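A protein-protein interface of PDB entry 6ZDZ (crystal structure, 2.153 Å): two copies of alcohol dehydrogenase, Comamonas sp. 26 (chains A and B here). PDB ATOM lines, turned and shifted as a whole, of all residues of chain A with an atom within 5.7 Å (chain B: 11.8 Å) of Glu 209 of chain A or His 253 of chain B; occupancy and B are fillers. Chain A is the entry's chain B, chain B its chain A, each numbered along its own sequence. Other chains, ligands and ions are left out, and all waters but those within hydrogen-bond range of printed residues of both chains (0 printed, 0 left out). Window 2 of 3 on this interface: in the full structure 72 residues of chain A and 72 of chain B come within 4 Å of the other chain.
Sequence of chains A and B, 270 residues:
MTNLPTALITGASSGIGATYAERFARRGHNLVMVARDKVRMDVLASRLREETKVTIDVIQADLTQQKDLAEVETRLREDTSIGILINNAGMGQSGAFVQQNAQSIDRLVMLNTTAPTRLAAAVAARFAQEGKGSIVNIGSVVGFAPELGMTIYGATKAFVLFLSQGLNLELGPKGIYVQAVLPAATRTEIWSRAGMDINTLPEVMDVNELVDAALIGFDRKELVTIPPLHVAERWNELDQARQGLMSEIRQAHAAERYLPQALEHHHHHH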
ATOM      1  N   ARG A  23      16.797 -18.418   1.866  1.00  0.00           N
ATOM      2  CA  ARG A  23      16.560 -19.785   1.410  1.00  0.00           C
ATOM      3  C   ARG A  23      16.411 -19.852  -0.106  1.00  0.00           C
ATOM      4  O   ARG A  23      17.003 -20.720  -0.759  1.00  0.00           O
ATOM      5  CB  ARG A  23      15.317 -20.361   2.089  1.00  0.00           C
ATOM      6  CG  ARG A  23      15.402 -20.472   3.599  1.00  0.00           C
ATOM      7  CD  ARG A  23      16.533 -21.388   4.026  1.00  0.00           C
ATOM      8  NE  ARG A  23      16.500 -21.660   5.459  1.00  0.00           N
ATOM      9  CZ  ARG A  23      17.211 -20.995   6.364  1.00  0.00           C
ATOM     10  NH1 ARG A  23      18.017 -20.012   5.988  1.00  0.00           N
ATOM     11  NH2 ARG A  23      17.117 -21.317   7.646  1.00  0.00           N
ATOM     12  N   GLU A 203       9.349 -19.353  25.352  1.00  0.00           N
ATOM     13  CA  GLU A 203      10.226 -19.827  24.287  1.00  0.00           C
ATOM     14  C   GLU A 203       9.446 -19.941  22.983  1.00  0.00           C
ATOM     15  O   GLU A 203       8.496 -20.724  22.884  1.00  0.00           O
ATOM     16  CB  GLU A 203      10.837 -21.174  24.665  1.00  0.00           C
ATOM     17  CG  GLU A 203      11.596 -21.847  23.536  1.00  0.00           C
ATOM     18  CD  GLU A 203      12.320 -23.100  23.988  1.00  0.00           C
ATOM     19  OE1 GLU A 203      12.373 -23.347  25.211  1.00  0.00           O
ATOM     20  OE2 GLU A 203      12.833 -23.838  23.121  1.00  0.00           O
ATOM     21  N   MET A 205       9.606 -20.180  18.481  1.00  0.00           N
ATOM     22  CA  MET A 205      10.290 -20.997  17.493  1.00  0.00           C
ATOM     23  C   MET A 205      11.388 -20.196  16.803  1.00  0.00           C
ATOM     24  O   MET A 205      11.276 -18.980  16.619  1.00  0.00           O
ATOM     25  CB  MET A 205       9.296 -21.519  16.454  1.00  0.00           C
ATOM     26  CG  MET A 205       9.825 -22.629  15.565  1.00  0.00           C
ATOM     27  SD  MET A 205       8.628 -23.096  14.301  1.00  0.00           S
ATOM     28  CE  MET A 205       7.195 -23.468  15.310  1.00  0.00           C
ATOM     29  N   ASP A 206      12.459 -20.888  16.427  1.00  0.00           N
ATOM     30  CA  ASP A 206      13.500 -20.262  15.626  1.00  0.00           C
ATOM     31  C   ASP A 206      12.953 -19.935  14.241  1.00  0.00           C
ATOM     32  O   ASP A 206      12.225 -20.730  13.641  1.00  0.00           O
ATOM     33  CB  ASP A 206      14.715 -21.182  15.519  1.00  0.00           C
ATOM     34  CG  ASP A 206      15.926 -20.493  14.912  1.00  0.00           C
ATOM     35  OD1 ASP A 206      15.829 -19.300  14.550  1.00  0.00           O
ATOM     36  OD2 ASP A 206      16.982 -21.149  14.798  1.00  0.00           O
ATOM     37  N   VAL A 207      13.304 -18.749  13.735  1.00  0.00           N
ATOM     38  CA  VAL A 207      12.805 -18.325  12.430  1.00  0.00           C
ATOM     39  C   VAL A 207      13.331 -19.232  11.326  1.00  0.00           C
ATOM     40  O   VAL A 207      12.681 -19.400  10.288  1.00  0.00           O
ATOM     41  CB  VAL A 207      13.155 -16.844  12.173  1.00  0.00           C
ATOM     42  CG1 VAL A 207      14.642 -16.672  11.890  1.00  0.00           C
ATOM     43  CG2 VAL A 207      12.318 -16.289  11.032  1.00  0.00           C
ATOM     44  N   ASN A 208      14.503 -19.838  11.529  1.00  0.00           N
ATOM     45  CA  ASN A 208      15.024 -20.780  10.546  1.00  0.00           C
ATOM     46  C   ASN A 208      14.206 -22.067  10.530  1.00  0.00           C
ATOM     47  O   ASN A 208      13.944 -22.626   9.460  1.00  0.00           O
ATOM     48  CB  ASN A 208      16.497 -21.075  10.827  1.00  0.00           C
ATOM     49  CG  ASN A 208      17.379 -19.855  10.641  1.00  0.00           C
ATOM     50  OD1 ASN A 208      17.504 -19.328   9.536  1.00  0.00           O
ATOM     51  ND2 ASN A 208      17.995 -19.401  11.726  1.00  0.00           N
ATOM     52  N   GLU A 209      13.803 -22.553  11.707  1.00  0.00           N
ATOM     53  CA  GLU A 209      12.909 -23.706  11.768  1.00  0.00           C
ATOM     54  C   GLU A 209      11.596 -23.421  11.050  1.00  0.00           C
ATOM     55  O   GLU A 209      11.094 -24.259  10.291  1.00  0.00           O
ATOM     56  CB  GLU A 209      12.634 -24.088  13.222  1.00  0.00           C
ATOM     57  CG  GLU A 209      13.664 -24.994  13.861  1.00  0.00           C
ATOM     58  CD  GLU A 209      13.132 -25.655  15.118  1.00  0.00           C
ATOM     59  OE1 GLU A 209      12.036 -26.253  15.053  1.00  0.00           O
ATOM     60  OE2 GLU A 209      13.800 -25.573  16.170  1.00  0.00           O
ATOM     61  N   LEU A 210      11.024 -22.239  11.287  1.00  0.00           N
ATOM     62  CA  LEU A 210       9.715 -21.913  10.730  1.00  0.00           C
ATOM     63  C   LEU A 210       9.747 -21.889   9.207  1.00  0.00           C
ATOM     64  O   LEU A 210       8.868 -22.455   8.548  1.00  0.00           O
ATOM     65  CB  LEU A 210       9.242 -20.569  11.278  1.00  0.00           C
ATOM     66  CG  LEU A 210       7.961 -20.022  10.655  1.00  0.00           C
ATOM     67  CD1 LEU A 210       6.757 -20.818  11.123  1.00  0.00           C
ATOM     68  CD2 LEU A 210       7.810 -18.559  10.997  1.00  0.00           C
ATOM     69  N   VAL A 211      10.756 -21.235   8.628  1.00  0.00           N
ATOM     70  CA  VAL A 211      10.805 -21.108   7.176  1.00  0.00           C
ATOM     71  C   VAL A 211      11.204 -22.433   6.538  1.00  0.00           C
ATOM     72  O   VAL A 211      10.697 -22.800   5.471  1.00  0.00           O
ATOM     73  CB  VAL A 211      11.755 -19.965   6.772  1.00  0.00           C
ATOM     74  CG1 VAL A 211      11.926 -19.914   5.260  1.00  0.00           C
ATOM     75  CG2 VAL A 211      11.223 -18.639   7.291  1.00  0.00           C
ATOM     76  N   ASP A 212      12.104 -23.179   7.184  1.00  0.00           N
ATOM     77  CA  ASP A 212      12.445 -24.509   6.687  1.00  0.00           C
ATOM     78  C   ASP A 212      11.230 -25.427   6.713  1.00  0.00           C
ATOM     79  O   ASP A 212      11.028 -26.230   5.794  1.00  0.00           O
ATOM     80  CB  ASP A 212      13.586 -25.109   7.508  1.00  0.00           C
ATOM     81  CG  ASP A 212      14.924 -24.459   7.211  1.00  0.00           C
ATOM     82  OD1 ASP A 212      14.977 -23.574   6.332  1.00  0.00           O
ATOM     83  OD2 ASP A 212      15.926 -24.836   7.857  1.00  0.00           O
ATOM     84  N   ALA A 213      10.412 -25.326   7.764  1.00  0.00           N
ATOM     85  CA  ALA A 213       9.186 -26.114   7.824  1.00  0.00           C
ATOM     86  C   ALA A 213       8.187 -25.665   6.765  1.00  0.00           C
ATOM     87  O   ALA A 213       7.539 -26.498   6.121  1.00  0.00           O
ATOM     88  CB  ALA A 213       8.571 -26.018   9.219  1.00  0.00           C
ATOM     89  N   ALA A 214       8.046 -24.350   6.577  1.00  0.00           N
ATOM     90  CA  ALA A 214       7.122 -23.837   5.570  1.00  0.00           C
ATOM     91  C   ALA A 214       7.546 -24.247   4.165  1.00  0.00           C
ATOM     92  O   ALA A 214       6.697 -24.501   3.301  1.00  0.00           O
ATOM     93  CB  ALA A 214       7.024 -22.317   5.675  1.00  0.00           C
ATOM     94  N   PRO A 227       3.266 -24.867  10.916  1.00  0.00           N
ATOM     95  CA  PRO A 227       4.395 -25.540  11.588  1.00  0.00           C
ATOM     96  C   PRO A 227       4.162 -25.768  13.076  1.00  0.00           C
ATOM     97  O   PRO A 227       4.465 -26.863  13.574  1.00  0.00           O
ATOM     98  CB  PRO A 227       5.571 -24.583  11.340  1.00  0.00           C
ATOM     99  CG  PRO A 227       5.217 -23.910  10.052  1.00  0.00           C
ATOM    100  CD  PRO A 227       3.717 -23.751  10.066  1.00  0.00           C
ATOM    101  N   PRO A 228       3.641 -24.793  13.838  1.00  0.00           N
ATOM    102  CA  PRO A 228       3.475 -25.035  15.281  1.00  0.00           C
ATOM    103  C   PRO A 228       2.324 -25.964  15.640  1.00  0.00           C
ATOM    104  O   PRO A 228       2.120 -26.227  16.830  1.00  0.00           O
ATOM    105  CB  PRO A 228       3.239 -23.628  15.847  1.00  0.00           C
ATOM    106  CG  PRO A 228       2.611 -22.898  14.746  1.00  0.00           C
ATOM    107  CD  PRO A 228       3.277 -23.401  13.501  1.00  0.00           C
ATOM    108  N   SER B 247      -5.403 -25.919  21.089  1.00  0.00           N
ATOM    109  CA  SER B 247      -4.891 -26.745  22.175  1.00  0.00           C
ATOM    110  C   SER B 247      -3.691 -27.580  21.749  1.00  0.00           C
ATOM    111  O   SER B 247      -2.963 -28.080  22.613  1.00  0.00           O
ATOM    112  CB  SER B 247      -5.995 -27.661  22.707  1.00  0.00           C
ATOM    113  OG  SER B 247      -6.301 -28.687  21.777  1.00  0.00           O
ATOM    114  N   GLU B 248      -3.469 -27.742  20.443  1.00  0.00           N
ATOM    115  CA  GLU B 248      -2.336 -28.500  19.930  1.00  0.00           C
ATOM    116  C   GLU B 248      -1.245 -27.594  19.366  1.00  0.00           C
ATOM    117  O   GLU B 248      -0.368 -28.066  18.637  1.00  0.00           O
ATOM    118  CB  GLU B 248      -2.805 -29.493  18.864  1.00  0.00           C
ATOM    119  CG  GLU B 248      -3.844 -30.498  19.352  1.00  0.00           C
ATOM    120  CD  GLU B 248      -3.301 -31.491  20.366  1.00  0.00           C
ATOM    121  OE1 GLU B 248      -2.067 -31.553  20.559  1.00  0.00           O
ATOM    122  OE2 GLU B 248      -4.117 -32.210  20.982  1.00  0.00           O
ATOM    123  N   ILE B 249      -1.287 -26.302  19.680  1.00  0.00           N
ATOM    124  CA  ILE B 249      -0.263 -25.364  19.226  1.00  0.00           C
ATOM    125  C   ILE B 249       0.900 -25.404  20.212  1.00  0.00           C
ATOM    126  O   ILE B 249       0.761 -25.009  21.372  1.00  0.00           O
ATOM    127  CB  ILE B 249      -0.822 -23.944  19.086  1.00  0.00           C
ATOM    128  CG1 ILE B 249      -1.819 -23.875  17.928  1.00  0.00           C
ATOM    129  CG2 ILE B 249       0.308 -22.945  18.876  1.00  0.00           C
ATOM    130  CD1 ILE B 249      -1.211 -24.196  16.579  1.00  0.00           C
ATOM    131  N   ARG B 250       2.050 -25.892  19.751  1.00  0.00           N
ATOM    132  CA  ARG B 250       3.278 -25.927  20.538  1.00  0.00           C
ATOM    133  C   ARG B 250       4.328 -25.111  19.796  1.00  0.00           C
ATOM    134  O   ARG B 250       4.868 -25.562  18.779  1.00  0.00           O
ATOM    135  CB  ARG B 250       3.731 -27.364  20.785  1.00  0.00           C
ATOM    136  CG  ARG B 250       2.595 -28.261  21.251  1.00  0.00           C
ATOM    137  CD  ARG B 250       3.082 -29.479  22.010  1.00  0.00           C
ATOM    138  NE  ARG B 250       1.964 -30.333  22.398  1.00  0.00           N
ATOM    139  CZ  ARG B 250       2.061 -31.376  23.215  1.00  0.00           C
ATOM    140  NH1 ARG B 250       3.232 -31.704  23.744  1.00  0.00           N
ATOM    141  NH2 ARG B 250       0.983 -32.090  23.508  1.00  0.00           N
ATOM    142  N   GLN B 251       4.616 -23.914  20.310  1.00  0.00           N
ATOM    143  CA  GLN B 251       5.412 -22.927  19.592  1.00  0.00           C
ATOM    144  C   GLN B 251       6.912 -23.159  19.699  1.00  0.00           C
ATOM    145  O   GLN B 251       7.671 -22.485  18.996  1.00  0.00           O
ATOM    146  CB  GLN B 251       5.093 -21.523  20.113  1.00  0.00           C
ATOM    147  CG  GLN B 251       3.613 -21.215  20.239  1.00  0.00           C
ATOM    148  CD  GLN B 251       3.354 -19.752  20.535  1.00  0.00           C
ATOM    149  OE1 GLN B 251       4.266 -18.927  20.491  1.00  0.00           O
ATOM    150  NE2 GLN B 251       2.105 -19.423  20.844  1.00  0.00           N
ATOM    151  N   ALA B 252       7.362 -24.079  20.553  1.00  0.00           N
ATOM    152  CA  ALA B 252       8.798 -24.235  20.766  1.00  0.00           C
ATOM    153  C   ALA B 252       9.487 -24.815  19.537  1.00  0.00           C
ATOM    154  O   ALA B 252      10.598 -24.399  19.190  1.00  0.00           O
ATOM    155  CB  ALA B 252       9.058 -25.113  21.990  1.00  0.00           C
ATOM    156  N   HIS B 253       8.850 -25.771  18.865  1.00  0.00           N
ATOM    157  CA  HIS B 253       9.474 -26.433  17.731  1.00  0.00           C
ATOM    158  C   HIS B 253       8.416 -26.768  16.693  1.00  0.00           C
ATOM    159  O   HIS B 253       7.234 -26.918  17.014  1.00  0.00           O
ATOM    160  CB  HIS B 253      10.202 -27.711  18.165  1.00  0.00           C
ATOM    161  CG  HIS B 253      11.386 -27.463  19.045  1.00  0.00           C
ATOM    162  ND1 HIS B 253      12.549 -26.882  18.586  1.00  0.00           N
ATOM    163  CD2 HIS B 253      11.583 -27.711  20.362  1.00  0.00           C
ATOM    164  CE1 HIS B 253      13.413 -26.788  19.581  1.00  0.00           C
ATOM    165  NE2 HIS B 253      12.852 -27.283  20.669  1.00  0.00           N
ATOM    166  N   ALA B 254       8.855 -26.879  15.441  1.00  0.00           N
ATOM    167  CA  ALA B 254       7.968 -27.314  14.373  1.00  0.00           C
ATOM    168  C   ALA B 254       7.568 -28.770  14.583  1.00  0.00           C
ATOM    169  O   ALA B 254       8.290 -29.554  15.203  1.00  0.00           O
ATOM    170  CB  ALA B 254       8.642 -27.143  13.013  1.00  0.00           C
ATOM    171  N   ALA B 255       6.394 -29.124  14.063  1.00  0.00           N
ATOM    172  CA  ALA B 255       5.925 -30.500  14.144  1.00  0.00           C
ATOM    173  C   ALA B 255       6.902 -31.443  13.449  1.00  0.00           C
ATOM    174  O   ALA B 255       7.633 -31.053  12.534  1.00  0.00           O
ATOM    175  CB  ALA B 255       4.537 -30.628  13.518  1.00  0.00           C
ATOM    176  N   GLU B 256       6.910 -32.700  13.901  1.00  0.00           N
ATOM    177  CA  GLU B 256       7.857 -33.675  13.368  1.00  0.00           C
ATOM    178  C   GLU B 256       7.636 -33.931  11.883  1.00  0.00           C
ATOM    179  O   GLU B 256       8.575 -34.315  11.176  1.00  0.00           O
ATOM    180  CB  GLU B 256       7.765 -34.987  14.148  1.00  0.00           C
ATOM    181  CG  GLU B 256       8.147 -34.870  15.613  1.00  0.00           C
ATOM    182  CD  GLU B 256       8.076 -36.198  16.338  1.00  0.00           C
ATOM    183  OE1 GLU B 256       7.659 -37.197  15.712  1.00  0.00           O
ATOM    184  OE2 GLU B 256       8.437 -36.248  17.532  1.00  0.00           O
ATOM    185  N   ARG B 257       6.412 -33.725  11.391  1.00  0.00           N
ATOM    186  CA  ARG B 257       6.131 -33.937   9.976  1.00  0.00           C
ATOM    187  C   ARG B 257       6.844 -32.938   9.074  1.00  0.00           C
ATOM    188  O   ARG B 257       6.794 -33.092   7.850  1.00  0.00           O
ATOM    189  CB  ARG B 257       4.624 -33.874   9.722  1.00  0.00           C
ATOM    190  CG  ARG B 257       3.993 -32.534  10.060  1.00  0.00           C
ATOM    191  CD  ARG B 257       2.491 -32.555   9.826  1.00  0.00           C
ATOM    192  NE  ARG B 257       1.889 -31.240  10.017  1.00  0.00           N
ATOM    193  CZ  ARG B 257       1.476 -30.769  11.189  1.00  0.00           C
ATOM    194  NH1 ARG B 257       1.596 -31.509  12.282  1.00  0.00           N
ATOM    195  NH2 ARG B 257       0.940 -29.559  11.269  1.00  0.00           N
ATOM    196  N   TYR B 258       7.500 -31.923   9.641  1.00  0.00           N
ATOM    197  CA  TYR B 258       8.294 -30.970   8.876  1.00  0.00           C
ATOM    198  C   TYR B 258       9.784 -31.096   9.180  1.00  0.00           C
ATOM    199  O   TYR B 258      10.542 -30.147   8.956  1.00  0.00           O
ATOM    200  CB  TYR B 258       7.823 -29.540   9.145  1.00  0.00           C
ATOM    201  CG  TYR B 258       6.389 -29.271   8.745  1.00  0.00           C
ATOM    202  CD1 TYR B 258       5.431 -28.948   9.696  1.00  0.00           C
ATOM    203  CD2 TYR B 258       5.994 -29.341   7.416  1.00  0.00           C
ATOM    204  CE1 TYR B 258       4.119 -28.701   9.334  1.00  0.00           C
ATOM    205  CE2 TYR B 258       4.686 -29.098   7.045  1.00  0.00           C
ATOM    206  CZ  TYR B 258       3.752 -28.777   8.007  1.00  0.00           C
ATOM    207  OH  TYR B 258       2.447 -28.533   7.641  1.00  0.00           O
ATOM    208  N   LEU B 259      10.216 -32.248   9.683  1.00  0.00           N
ATOM    209  CA  LEU B 259      11.616 -32.458  10.030  1.00  0.00           C
ATOM    210  C   LEU B 259      12.202 -33.640   9.266  1.00  0.00           C
ATOM    211  O   LEU B 259      12.569 -34.653   9.859  1.00  0.00           O
ATOM    212  CB  LEU B 259      11.765 -32.680  11.537  1.00  0.00           C
ATOM    213  CG  LEU B 259      11.202 -31.580  12.442  1.00  0.00           C
ATOM    214  CD1 LEU B 259      11.283 -31.992  13.904  1.00  0.00           C
ATOM    215  CD2 LEU B 259      11.932 -30.268  12.209  1.00  0.00           C
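No position is printed for both chains.
Among the printed residues, merely in contact across the chains: Met 205 of chain A with Ala 252 of chain B (3.8 Å), Met 205 of chain A with His 253 of chain B (3.8 Å), Met 205 of chain A with Ala 254 of chain B (3.8 Å), Ala 213 of chain A with Ala 254 of chain B (3.96 Å), Ala 213 of chain A with Tyr 258 of chain B (3.5 Å), Pro 227 of chain A with Ala 254 of chain B (3.6 Å), Pro 227 of chain A with Tyr 258 of chain B (3.9 Å), Pro 228 of chain A with Glu 248 of chain B (3.6 Å) and Pro 228 of chain A with Ile 249 of chain B (3.5 Å).
Of the printed residues of chain B, Glu 209 of chain A touches His 253 and Ala 254.
Of chain A, only Met 205 (3.8 Å) and Glu 209 (3.0 Å) come within 4 Å of His 253 of chain B.
No residue of chain B comes within 4 Å of Asp 206 of chain A.
No residue of chain B comes within 4 Å of Val 207 of chain A.
No residue of chain B comes within 4 Å of Asn 208 of chain A.
No residue of chain B comes within 4 Å of Leu 210 of chain A.
No residue of chain B comes within 4 Å of Asp 212 of chain A.
Ala 213 of chain A touches two residues of chain B.
Of chain B, only Ala 254, Ala 255 and Tyr 258 come within 4 Å of Pro 227 of chain A.
Printed residues of chain B within 4 Å of Pro 228 of chain A: Glu 248, Ile 249 and Arg 250.
Of the printed residues of chain A, Arg 250 of chain B touches Pro 228 (2.9 Å).
Of the printed residues of chain A, Ile 249 of chain B touches Pro 228.
Printed residues of chain A within 4 Å of Ala 252 of chain B: Met 205 (3.8 Å).
Ser 247 of chain B touches none of the printed residues of chain A.
Ala 214 of chain A touches none of the printed residues of chain B.
The nearest residue of chain B that does not touch Glu 209 of chain A is Ala 252 of chain B (4.6 Å).
The backbone NH (N) of Arg 250 of chain B lies within hydrogen-bond range of the backbone carbonyl oxygen (O) of Pro 228 of chain A.
The backbone NH (N) of Met 205 of chain A sits at hydrogen-bond distance from the backbone carbonyl oxygen (O) of Gln 251 of chain B (3.1 Å).
A ring nitrogen (ND1) of His 253 of chain B sits at hydrogen-bond distance from the side-chain carboxylate of Glu 209 of chain A (3.0 Å).
The backbone NH (N) of Ala 254 of chain B is in hydrogen-bond range of the side-chain carboxylate (OE1) of Glu 209 of chain A (3.3 Å).
N of Ala 255 of chain B lies within hydrogen-bond range of O of Pro 227 of chain A (3.0 Å).
Printed residues of chain A that touch a printed residue of chain B: Met 205, Glu 209, Ala 213, Pro 227 and Pro 228.
Hydrophobic or aromatic side chains of chain A that line the printed part of chain B: Met 205, Ala 213 and Pro 228.
Hydrophobic or aromatic side chains of chain B that line the printed part of chain A: Ile 249, His 253, Ala 254, Ala 255 and Tyr 258.
Among the printed residues, 14 pairs touch across the chains.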
